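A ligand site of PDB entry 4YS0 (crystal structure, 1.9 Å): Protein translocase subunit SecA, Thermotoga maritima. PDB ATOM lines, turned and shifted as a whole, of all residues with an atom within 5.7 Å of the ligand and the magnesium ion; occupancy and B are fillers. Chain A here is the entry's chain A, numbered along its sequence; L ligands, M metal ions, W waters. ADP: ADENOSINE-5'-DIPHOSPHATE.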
ATOM      1  N   GLY A  73     -29.778   9.181  -3.553  1.00  0.00           N
ATOM      2  CA  GLY A  73     -30.848   8.579  -2.775  1.00  0.00           C
ATOM      3  C   GLY A  73     -30.341   7.366  -1.996  1.00  0.00           C
ATOM      4  O   GLY A  73     -31.118   6.504  -1.625  1.00  0.00           O
ATOM      5  N   MET A  74     -29.038   7.342  -1.740  1.00  0.00           N
ATOM      6  CA  MET A  74     -28.423   6.294  -0.931  1.00  0.00           C
ATOM      7  C   MET A  74     -27.646   6.897   0.216  1.00  0.00           C
ATOM      8  O   MET A  74     -26.728   7.681  -0.001  1.00  0.00           O
ATOM      9  CB  MET A  74     -27.487   5.424  -1.802  1.00  0.00           C
ATOM     10  CG  MET A  74     -28.225   4.646  -2.878  1.00  0.00           C
ATOM     11  SD  MET A  74     -27.138   3.434  -3.701  1.00  0.00           S
ATOM     12  CE  MET A  74     -25.717   4.449  -4.018  1.00  0.00           C
ATOM     13  N   ARG A  75     -28.017   6.541   1.445  1.00  0.00           N
ATOM     14  CA  ARG A  75     -27.276   6.998   2.609  1.00  0.00           C
ATOM     15  C   ARG A  75     -26.371   5.876   3.153  1.00  0.00           C
ATOM     16  O   ARG A  75     -26.877   4.851   3.626  1.00  0.00           O
ATOM     17  CB  ARG A  75     -28.252   7.493   3.706  1.00  0.00           C
ATOM     18  CG  ARG A  75     -27.586   7.891   5.007  1.00  0.00           C
ATOM     19  CD  ARG A  75     -28.651   8.193   6.086  1.00  0.00           C
ATOM     20  NE  ARG A  75     -28.039   8.378   7.393  1.00  0.00           N
ATOM     21  CZ  ARG A  75     -27.746   7.389   8.224  1.00  0.00           C
ATOM     22  NH1 ARG A  75     -27.987   6.135   7.870  1.00  0.00           N
ATOM     23  NH2 ARG A  75     -27.198   7.652   9.401  1.00  0.00           N
ATOM     24  N   PRO A  76     -25.036   6.057   3.071  1.00  0.00           N
ATOM     25  CA  PRO A  76     -24.098   5.056   3.580  1.00  0.00           C
ATOM     26  C   PRO A  76     -24.442   4.623   4.989  1.00  0.00           C
ATOM     27  O   PRO A  76     -24.636   5.439   5.897  1.00  0.00           O
ATOM     28  CB  PRO A  76     -22.753   5.790   3.538  1.00  0.00           C
ATOM     29  CG  PRO A  76     -22.876   6.702   2.390  1.00  0.00           C
ATOM     30  CD  PRO A  76     -24.340   7.100   2.288  1.00  0.00           C
ATOM     31  N   PHE A  77     -24.571   3.318   5.153  1.00  0.00           N
ATOM     32  CA  PHE A  77     -24.857   2.708   6.442  1.00  0.00           C
ATOM     33  C   PHE A  77     -23.667   2.924   7.334  1.00  0.00           C
ATOM     34  O   PHE A  77     -22.563   3.183   6.849  1.00  0.00           O
ATOM     35  CB  PHE A  77     -25.154   1.200   6.301  1.00  0.00           C
ATOM     36  CG  PHE A  77     -26.210   0.887   5.277  1.00  0.00           C
ATOM     37  CD1 PHE A  77     -27.389   1.627   5.239  1.00  0.00           C
ATOM     38  CD2 PHE A  77     -26.033  -0.135   4.355  1.00  0.00           C
ATOM     39  CE1 PHE A  77     -28.355   1.362   4.299  1.00  0.00           C
ATOM     40  CE2 PHE A  77     -27.015  -0.404   3.396  1.00  0.00           C
ATOM     41  CZ  PHE A  77     -28.178   0.340   3.376  1.00  0.00           C
ATOM     42  N   GLN A  80     -20.703   0.933   6.288  1.00  0.00           N
ATOM     43  CA  GLN A  80     -19.996   1.461   5.127  1.00  0.00           C
ATOM     44  C   GLN A  80     -19.044   2.591   5.549  1.00  0.00           C
ATOM     45  O   GLN A  80     -17.903   2.661   5.077  1.00  0.00           O
ATOM     46  CB  GLN A  80     -20.967   1.964   4.078  1.00  0.00           C
ATOM     47  CG  GLN A  80     -21.620   0.824   3.263  1.00  0.00           C
ATOM     48  CD  GLN A  80     -22.718   1.339   2.354  1.00  0.00           C
ATOM     49  OE1 GLN A  80     -23.708   1.910   2.819  1.00  0.00           O
ATOM     50  NE2 GLN A  80     -22.554   1.154   1.044  1.00  0.00           N
ATOM     51  N   MET A  95     -15.495  -6.341   3.608  1.00  0.00           N
ATOM     52  CA  MET A  95     -16.931  -6.152   3.651  1.00  0.00           C
ATOM     53  C   MET A  95     -17.515  -7.186   2.717  1.00  0.00           C
ATOM     54  O   MET A  95     -17.100  -7.256   1.546  1.00  0.00           O
ATOM     55  CB  MET A  95     -17.333  -4.754   3.208  1.00  0.00           C
ATOM     56  CG  MET A  95     -16.828  -3.652   4.162  1.00  0.00           C
ATOM     57  SD  MET A  95     -16.971  -2.013   3.427  1.00  0.00           S
ATOM     58  CE  MET A  95     -18.728  -1.872   3.154  1.00  0.00           C
ATOM     59  N   LYS A  96     -18.465  -7.971   3.206  1.00  0.00           N
ATOM     60  CA  LYS A  96     -18.968  -9.080   2.384  1.00  0.00           C
ATOM     61  C   LYS A  96     -19.649  -8.578   1.105  1.00  0.00           C
ATOM     62  O   LYS A  96     -19.996  -7.386   0.990  1.00  0.00           O
ATOM     63  CB  LYS A  96     -19.955  -9.943   3.192  1.00  0.00           C
ATOM     64  CG  LYS A  96     -19.333 -10.589   4.458  1.00  0.00           C
ATOM     65  CD  LYS A  96     -18.230 -11.590   4.059  1.00  0.00           C
ATOM     66  CE  LYS A  96     -17.568 -12.246   5.294  1.00  0.00           C
ATOM     67  NZ  LYS A  96     -16.350 -12.986   4.866  1.00  0.00           N
ATOM     68  N   THR A  97     -19.834  -9.504   0.168  1.00  0.00           N
ATOM     69  CA  THR A  97     -20.510  -9.223  -1.092  1.00  0.00           C
ATOM     70  C   THR A  97     -21.891  -8.622  -0.816  1.00  0.00           C
ATOM     71  O   THR A  97     -22.630  -9.107   0.043  1.00  0.00           O
ATOM     72  CB  THR A  97     -20.627 -10.513  -1.947  1.00  0.00           C
ATOM     73  OG1 THR A  97     -19.314 -10.917  -2.339  1.00  0.00           O
ATOM     74  CG2 THR A  97     -21.495 -10.282  -3.200  1.00  0.00           C
ATOM     75  N   GLY A  98     -22.205  -7.550  -1.515  1.00  0.00           N
ATOM     76  CA  GLY A  98     -23.484  -6.890  -1.329  1.00  0.00           C
ATOM     77  C   GLY A  98     -23.519  -5.866  -0.188  1.00  0.00           C
ATOM     78  O   GLY A  98     -24.562  -5.249   0.044  1.00  0.00           O
ATOM     79  N   GLU A  99     -22.415  -5.666   0.507  1.00  0.00           N
ATOM     80  CA  GLU A  99     -22.410  -4.658   1.588  1.00  0.00           C
ATOM     81  C   GLU A  99     -22.254  -3.217   1.101  1.00  0.00           C
ATOM     82  O   GLU A  99     -22.322  -2.295   1.908  1.00  0.00           O
ATOM     83  CB  GLU A  99     -21.300  -4.984   2.597  1.00  0.00           C
ATOM     84  CG  GLU A  99     -21.607  -6.240   3.402  1.00  0.00           C
ATOM     85  CD  GLU A  99     -22.843  -6.079   4.288  1.00  0.00           C
ATOM     86  OE1 GLU A  99     -22.845  -5.134   5.117  1.00  0.00           O
ATOM     87  OE2 GLU A  99     -23.787  -6.891   4.147  1.00  0.00           O
ATOM     88  N   GLY A 100     -22.058  -3.034  -0.208  1.00  0.00           N
ATOM     89  CA  GLY A 100     -21.935  -1.692  -0.756  1.00  0.00           C
ATOM     90  C   GLY A 100     -20.535  -1.100  -0.639  1.00  0.00           C
ATOM     91  O   GLY A 100     -20.346   0.056  -0.253  1.00  0.00           O
ATOM     92  N   LYS A 101     -19.534  -1.898  -0.975  1.00  0.00           N
ATOM     93  CA  LYS A 101     -18.149  -1.421  -1.047  1.00  0.00           C
ATOM     94  C   LYS A 101     -17.970  -0.243  -2.016  1.00  0.00           C
ATOM     95  O   LYS A 101     -17.203   0.671  -1.742  1.00  0.00           O
ATOM     96  CB  LYS A 101     -17.220  -2.586  -1.459  1.00  0.00           C
ATOM     97  CG  LYS A 101     -17.043  -3.664  -0.352  1.00  0.00           C
ATOM     98  CD  LYS A 101     -16.059  -4.791  -0.771  1.00  0.00           C
ATOM     99  CE  LYS A 101     -16.724  -5.842  -1.680  1.00  0.00           C
ATOM    100  NZ  LYS A 101     -17.922  -6.472  -1.033  1.00  0.00           N
ATOM    101  N   THR A 102     -18.680  -0.285  -3.138  1.00  0.00           N
ATOM    102  CA  THR A 102     -18.583   0.773  -4.148  1.00  0.00           C
ATOM    103  C   THR A 102     -18.856   2.150  -3.519  1.00  0.00           C
ATOM    104  O   THR A 102     -18.082   3.103  -3.708  1.00  0.00           O
ATOM    105  CB  THR A 102     -19.590   0.587  -5.295  1.00  0.00           C
ATOM    106  OG1 THR A 102     -19.581  -0.788  -5.748  1.00  0.00           O
ATOM    107  CG2 THR A 102     -19.254   1.561  -6.469  1.00  0.00           C
ATOM    108  N   LEU A 103     -19.926   2.225  -2.734  1.00  0.00           N
ATOM    109  CA  LEU A 103     -20.307   3.475  -2.060  1.00  0.00           C
ATOM    110  C   LEU A 103     -19.427   3.729  -0.810  1.00  0.00           C
ATOM    111  O   LEU A 103     -19.124   4.885  -0.488  1.00  0.00           O
ATOM    112  CB  LEU A 103     -21.792   3.442  -1.696  1.00  0.00           C
ATOM    113  CG  LEU A 103     -22.350   4.668  -0.957  1.00  0.00           C
ATOM    114  CD1 LEU A 103     -22.088   5.974  -1.719  1.00  0.00           C
ATOM    115  CD2 LEU A 103     -23.833   4.465  -0.702  1.00  0.00           C
ATOM    116  N   ARG A 131     -18.735   1.551 -14.811  1.00  0.00           N
ATOM    117  CA  ARG A 131     -19.935   1.457 -13.979  1.00  0.00           C
ATOM    118  C   ARG A 131     -19.787   2.219 -12.655  1.00  0.00           C
ATOM    119  O   ARG A 131     -20.641   3.056 -12.321  1.00  0.00           O
ATOM    120  CB  ARG A 131     -20.299  -0.015 -13.701  1.00  0.00           C
ATOM    121  CG  ARG A 131     -21.648  -0.236 -12.997  1.00  0.00           C
ATOM    122  CD  ARG A 131     -21.684  -1.606 -12.255  1.00  0.00           C
ATOM    123  NE  ARG A 131     -20.860  -1.548 -11.027  1.00  0.00           N
ATOM    124  CZ  ARG A 131     -20.886  -2.465 -10.075  1.00  0.00           C
ATOM    125  NH1 ARG A 131     -21.676  -3.527 -10.207  1.00  0.00           N
ATOM    126  NH2 ARG A 131     -20.110  -2.351  -8.997  1.00  0.00           N
ATOM    127  N   TRP A 135     -21.755   5.491 -11.530  1.00  0.00           N
ATOM    128  CA  TRP A 135     -22.683   5.265 -10.429  1.00  0.00           C
ATOM    129  C   TRP A 135     -22.371   6.205  -9.259  1.00  0.00           C
ATOM    130  O   TRP A 135     -23.278   6.866  -8.722  1.00  0.00           O
ATOM    131  CB  TRP A 135     -22.632   3.787 -10.037  1.00  0.00           C
ATOM    132  CG  TRP A 135     -23.616   3.311  -9.027  1.00  0.00           C
ATOM    133  CD1 TRP A 135     -24.783   3.915  -8.633  1.00  0.00           C
ATOM    134  CD2 TRP A 135     -23.513   2.103  -8.260  1.00  0.00           C
ATOM    135  NE1 TRP A 135     -25.404   3.145  -7.650  1.00  0.00           N
ATOM    136  CE2 TRP A 135     -24.635   2.037  -7.411  1.00  0.00           C
ATOM    137  CE3 TRP A 135     -22.545   1.081  -8.186  1.00  0.00           C
ATOM    138  CZ2 TRP A 135     -24.832   0.982  -6.516  1.00  0.00           C
ATOM    139  CZ3 TRP A 135     -22.747   0.037  -7.311  1.00  0.00           C
ATOM    140  CH2 TRP A 135     -23.880  -0.013  -6.491  1.00  0.00           C
ATOM    141  N   GLU A 185     -33.408   4.243   6.829  1.00  0.00           N
ATOM    142  CA  GLU A 185     -32.038   3.940   6.422  1.00  0.00           C
ATOM    143  C   GLU A 185     -31.994   3.808   4.925  1.00  0.00           C
ATOM    144  O   GLU A 185     -30.962   4.019   4.300  1.00  0.00           O
ATOM    145  CB  GLU A 185     -31.535   2.657   7.080  1.00  0.00           C
ATOM    146  CG  GLU A 185     -30.715   2.856   8.325  1.00  0.00           C
ATOM    147  CD  GLU A 185     -29.851   1.647   8.628  1.00  0.00           C
ATOM    148  OE1 GLU A 185     -30.214   0.544   8.198  1.00  0.00           O
ATOM    149  OE2 GLU A 185     -28.786   1.804   9.282  1.00  0.00           O
ATOM    150  N   VAL A 186     -33.128   3.400   4.357  1.00  0.00           N
ATOM    151  CA  VAL A 186     -33.231   3.077   2.960  1.00  0.00           C
ATOM    152  C   VAL A 186     -34.494   3.708   2.383  1.00  0.00           C
ATOM    153  O   VAL A 186     -35.542   3.728   3.028  1.00  0.00           O
ATOM    154  CB  VAL A 186     -33.231   1.529   2.738  1.00  0.00           C
ATOM    155  CG1 VAL A 186     -33.595   1.173   1.338  1.00  0.00           C
ATOM    156  CG2 VAL A 186     -31.877   0.920   3.125  1.00  0.00           C
ATOM    157  N   ASP A 252     -10.344  -2.332  -5.274  1.00  0.00           N
ATOM    158  CA  ASP A 252     -11.589  -3.113  -5.182  1.00  0.00           C
ATOM    159  C   ASP A 252     -11.295  -4.576  -5.578  1.00  0.00           C
ATOM    160  O   ASP A 252     -10.302  -4.825  -6.252  1.00  0.00           O
ATOM    161  CB  ASP A 252     -12.662  -2.486  -6.072  1.00  0.00           C
ATOM    162  CG  ASP A 252     -14.083  -2.851  -5.644  1.00  0.00           C
ATOM    163  OD1 ASP A 252     -14.292  -3.700  -4.743  1.00  0.00           O
ATOM    164  OD2 ASP A 252     -15.014  -2.273  -6.250  1.00  0.00           O
ATOM    165  N   GLU A 253     -12.124  -5.521  -5.142  1.00  0.00           N
ATOM    166  CA  GLU A 253     -11.863  -6.964  -5.363  1.00  0.00           C
ATOM    167  C   GLU A 253     -10.401  -7.285  -5.015  1.00  0.00           C
ATOM    168  O   GLU A 253      -9.681  -7.929  -5.795  1.00  0.00           O
ATOM    169  CB  GLU A 253     -12.158  -7.359  -6.816  1.00  0.00           C
ATOM    170  CG  GLU A 253     -13.491  -6.834  -7.373  1.00  0.00           C
ATOM    171  CD  GLU A 253     -14.685  -7.554  -6.771  1.00  0.00           C
ATOM    172  OE1 GLU A 253     -14.486  -8.559  -6.040  1.00  0.00           O
ATOM    173  OE2 GLU A 253     -15.822  -7.163  -7.082  1.00  0.00           O
ATOM    174  N   GLY A 535     -19.223  -8.787  -9.103  1.00  0.00           N
ATOM    175  CA  GLY A 535     -19.531  -7.408  -8.766  1.00  0.00           C
ATOM    176  C   GLY A 535     -20.938  -6.917  -9.049  1.00  0.00           C
ATOM    177  O   GLY A 535     -21.304  -5.828  -8.597  1.00  0.00           O
ATOM    178  N   THR A 536     -21.724  -7.706  -9.802  1.00  0.00           N
ATOM    179  CA  THR A 536     -23.137  -7.363 -10.034  1.00  0.00           C
ATOM    180  C   THR A 536     -24.009  -7.931  -8.914  1.00  0.00           C
ATOM    181  O   THR A 536     -24.009  -9.138  -8.659  1.00  0.00           O
ATOM    182  CB  THR A 536     -23.647  -7.904 -11.403  1.00  0.00           C
ATOM    183  OG1 THR A 536     -22.949  -7.237 -12.465  1.00  0.00           O
ATOM    184  CG2 THR A 536     -25.185  -7.691 -11.573  1.00  0.00           C
ATOM    185  N   ASP A 537     -24.788  -7.069  -8.282  1.00  0.00           N
ATOM    186  CA  ASP A 537     -25.702  -7.489  -7.227  1.00  0.00           C
ATOM    187  C   ASP A 537     -26.810  -8.413  -7.786  1.00  0.00           C
ATOM    188  O   ASP A 537     -27.387  -8.127  -8.827  1.00  0.00           O
ATOM    189  CB  ASP A 537     -26.307  -6.249  -6.543  1.00  0.00           C
ATOM    190  CG  ASP A 537     -27.138  -6.593  -5.314  1.00  0.00           C
ATOM    191  OD1 ASP A 537     -26.777  -7.533  -4.565  1.00  0.00           O
ATOM    192  OD2 ASP A 537     -28.126  -5.880  -5.090  1.00  0.00           O
ATOM    193  N   LYS A 539     -30.285  -9.472  -6.921  1.00  0.00           N
ATOM    194  CA  LYS A 539     -31.448  -9.265  -6.068  1.00  0.00           C
ATOM    195  C   LYS A 539     -32.399 -10.458  -6.224  1.00  0.00           C
ATOM    196  O   LYS A 539     -32.453 -11.093  -7.276  1.00  0.00           O
ATOM    197  CB  LYS A 539     -32.126  -7.938  -6.433  1.00  0.00           C
ATOM    198  CG  LYS A 539     -31.209  -6.739  -6.199  1.00  0.00           C
ATOM    199  CD  LYS A 539     -31.861  -5.395  -6.545  1.00  0.00           C
ATOM    200  CE  LYS A 539     -30.908  -4.245  -6.196  1.00  0.00           C
ATOM    201  NZ  LYS A 539     -31.567  -2.923  -6.349  1.00  0.00           N
ATOM    202  N   ARG A 573     -27.087 -11.841   0.507  1.00  0.00           N
ATOM    203  CA  ARG A 573     -26.663 -10.432   0.576  1.00  0.00           C
ATOM    204  C   ARG A 573     -27.698  -9.588   1.362  1.00  0.00           C
ATOM    205  O   ARG A 573     -28.908  -9.824   1.275  1.00  0.00           O
ATOM    206  CB  ARG A 573     -26.534  -9.877  -0.847  1.00  0.00           C
ATOM    207  CG  ARG A 573     -27.877 -10.155  -1.519  1.00  0.00           C
ATOM    208  CD  ARG A 573     -28.368  -9.397  -2.696  1.00  0.00           C
ATOM    209  NE  ARG A 573     -28.499  -7.947  -2.627  1.00  0.00           N
ATOM    210  CZ  ARG A 573     -29.437  -7.246  -1.988  1.00  0.00           C
ATOM    211  NH1 ARG A 573     -30.350  -7.808  -1.209  1.00  0.00           N
ATOM    212  NH2 ARG A 573     -29.412  -5.932  -2.118  1.00  0.00           N
ATOM    213  N   GLN A 574     -27.216  -8.617   2.150  1.00  0.00           N
ATOM    214  CA  GLN A 574     -28.073  -7.707   2.899  1.00  0.00           C
ATOM    215  C   GLN A 574     -29.152  -8.433   3.706  1.00  0.00           C
ATOM    216  O   GLN A 574     -30.321  -8.035   3.733  1.00  0.00           O
ATOM    217  CB  GLN A 574     -28.709  -6.681   1.960  1.00  0.00           C
ATOM    218  CG  GLN A 574     -27.725  -5.653   1.429  1.00  0.00           C
ATOM    219  CD  GLN A 574     -27.228  -4.740   2.541  1.00  0.00           C
ATOM    220  OE1 GLN A 574     -27.907  -4.554   3.555  1.00  0.00           O
ATOM    221  NE2 GLN A 574     -26.039  -4.186   2.359  1.00  0.00           N
HETATM  222  PB  ADP L   1     -20.339  -4.858  -3.011  1.00  0.00           P
HETATM  223  O1B ADP L   1     -19.375  -4.176  -3.918  1.00  0.00           O
HETATM  224  O2B ADP L   1     -20.662  -6.248  -3.440  1.00  0.00           O
HETATM  225  O3B ADP L   1     -19.958  -4.690  -1.566  1.00  0.00           O
HETATM  226  PA  ADP L   1     -22.269  -3.043  -4.226  1.00  0.00           P
HETATM  227  O1A ADP L   1     -21.494  -1.751  -4.112  1.00  0.00           O
HETATM  228  O2A ADP L   1     -22.423  -3.727  -5.564  1.00  0.00           O
HETATM  229  O3A ADP L   1     -21.766  -4.095  -3.124  1.00  0.00           O
HETATM  230  O5' ADP L   1     -23.754  -2.795  -3.620  1.00  0.00           O
HETATM  231  C5' ADP L   1     -24.646  -3.892  -3.424  1.00  0.00           C
HETATM  232  C4' ADP L   1     -26.096  -3.394  -3.433  1.00  0.00           C
HETATM  233  O4' ADP L   1     -26.354  -2.533  -2.320  1.00  0.00           O
HETATM  234  C3' ADP L   1     -26.372  -2.554  -4.663  1.00  0.00           C
HETATM  235  O3' ADP L   1     -27.660  -2.938  -5.140  1.00  0.00           O
HETATM  236  C2' ADP L   1     -26.416  -1.130  -4.165  1.00  0.00           C
HETATM  237  O2' ADP L   1     -27.314  -0.352  -4.940  1.00  0.00           O
HETATM  238  C1' ADP L   1     -26.935  -1.310  -2.759  1.00  0.00           C
HETATM  239  N9  ADP L   1     -26.524  -0.310  -1.740  1.00  0.00           N
HETATM  240  C8  ADP L   1     -25.258  -0.173  -1.331  1.00  0.00           C
HETATM  241  N7  ADP L   1     -25.163   0.771  -0.373  1.00  0.00           N
HETATM  242  C5  ADP L   1     -26.412   1.211  -0.123  1.00  0.00           C
HETATM  243  C6  ADP L   1     -27.012   2.216   0.780  1.00  0.00           C
HETATM  244  N6  ADP L   1     -26.227   2.875   1.634  1.00  0.00           N
HETATM  245  N1  ADP L   1     -28.363   2.411   0.718  1.00  0.00           N
HETATM  246  C2  ADP L   1     -29.126   1.699  -0.139  1.00  0.00           C
HETATM  247  N3  ADP L   1     -28.644   0.778  -1.000  1.00  0.00           N
HETATM  248  C4  ADP L   1     -27.316   0.505  -1.032  1.00  0.00           C
HETATM  249 MG    MG M   1     -18.358  -4.573  -5.689  1.00  0.00          MG
HETATM  250  O   HOH W   1     -30.000  -0.659  -5.632  1.00  0.00           O
HETATM  251  O   HOH W   2     -16.454  -5.060  -4.843  1.00  0.00           O
HETATM  252  O   HOH W   3     -20.143  -4.216  -6.815  1.00  0.00           O
HETATM  253  O   HOH W   4     -30.648   0.023  -3.058  1.00  0.00           O
HETATM  254  O   HOH W   5     -18.961  -6.699  -5.390  1.00  0.00           O
HETATM  255  O   HOH W   6     -17.556  -2.632  -5.751  1.00  0.00           O
HETATM  256  O   HOH W   7     -22.443   0.531  -3.110  1.00  0.00           O
HETATM  257  O   HOH W   8     -17.385  -5.011  -7.721  1.00  0.00           O
HETATM  258  O   HOH W   9     -24.160  -3.826  -7.497  1.00  0.00           O
HETATM  259  O   HOH W  10     -29.754   4.333   1.719  1.00  0.00           O
HETATM  260  O   HOH W  11     -22.538  -6.790  -5.162  1.00  0.00           O
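Merely in contact with the magnesium ion: Thr 102 and Glu 253.
Of the 27 residues printed, 2 come within 4 Å of the magnesium ion.
The magnesium ion is bound by O1B of the ligand, water W6, water W2, water W3, water W5 and water W8.
The backbone NH (N) of Phe 77 is in hydrogen-bond range of the side-chain amide oxygen (OE1) of Gln 80, 2.9 Å away.
The backbone carbonyl oxygen (O) of Gly 535 lies within hydrogen-bond range of the guanidinium group (NH1) of Arg 131, 2.8 Å away.
The backbone carbonyl oxygen (O) of Gly 98 lies within hydrogen-bond range of the side-chain amide nitrogen (NE2) of Gln 574.
NE2 of Gln 80 lies within hydrogen-bond range of O of Gly 100 (2.8 Å).
OD1 of Asp 537 is in salt-bridge range of NE of Arg 573 (2.6 Å).
NZ of Lys 101 sits at hydrogen-bond distance from O of Met 95.
The side-chain amino group of Lys 101 lies within hydrogen-bond range of the backbone carbonyl oxygen of Lys 96 (3.0 Å).
Water W3 lies within hydrogen-bond range of O2A of the ligand (2.6 Å), O of Gly 535 (2.7 Å) and NH2 of Arg 131 (2.9 Å).
Water W6 bridges OD2 of Asp 252 (2.6 Å) and OG1 of Thr 102 (2.7 Å).
Water W2 lies within hydrogen-bond range of OD1 of Asp 252 (2.6 Å) and OE2 of Glu 253 (3.1 Å).
Water W10 lies within hydrogen-bond range of N1 of the ligand, N of Arg 75 and O of Glu 185.
Water W9 bridges O2A of the ligand (2.6 Å) and N of Asp 537 (3.4 Å).
Water W1 bridges O2' of the ligand (2.8 Å) and NZ of Lys 539 (2.8 Å).
The backbone NH (N) of Glu 99 lies within hydrogen-bond range of an oxygen (O3B) of the ligand, 3.4 Å away.
The backbone NH of Gly 98 sits at hydrogen-bond distance from an oxygen (O2B) of the ligand (2.8 Å).
OG1 of Thr 102 sits at hydrogen-bond distance from O1A of the ligand (2.7 Å).
O3B of the ligand is in hydrogen-bond range of N of Gly 100 (3.0 Å).
N of Thr 102 lies close to O1A of the ligand, at 3.3 Å.
O3B of the ligand lies within hydrogen-bond range of N of Lys 101.
A nitrogen (N6) of the ligand sits at hydrogen-bond distance from the backbone carbonyl oxygen (O) of Arg 75 (2.9 Å).
The side-chain amide oxygen of Gln 80 sits at hydrogen-bond distance from a nitrogen (N6) of the ligand.
An oxygen (O3') of the ligand lies within hydrogen-bond range of the side-chain carboxylate (OD2) of Asp 537, at 3.0 Å.
An oxygen (O3B) of the ligand lies within salt-bridge range of the side-chain amino group (NZ) of Lys 101 (2.8 Å).
Merely in contact with the ligand: Trp 135 (3.2 Å), Phe 77 (3.4 Å), Pro 76 (3.6 Å), Lys 539 (3.7 Å), Leu 103 (3.7 Å), Lys 96 (3.7 Å), Thr 97 (3.7 Å), Gly 535 (3.9 Å) and Met 74 (3.97 Å).
Hydrophobic or aromatic side chains that line the ligand: Met 74, Phe 77, Leu 103 and Trp 135.
Of the 27 residues printed, 17 come within 4 Å of the ligand.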
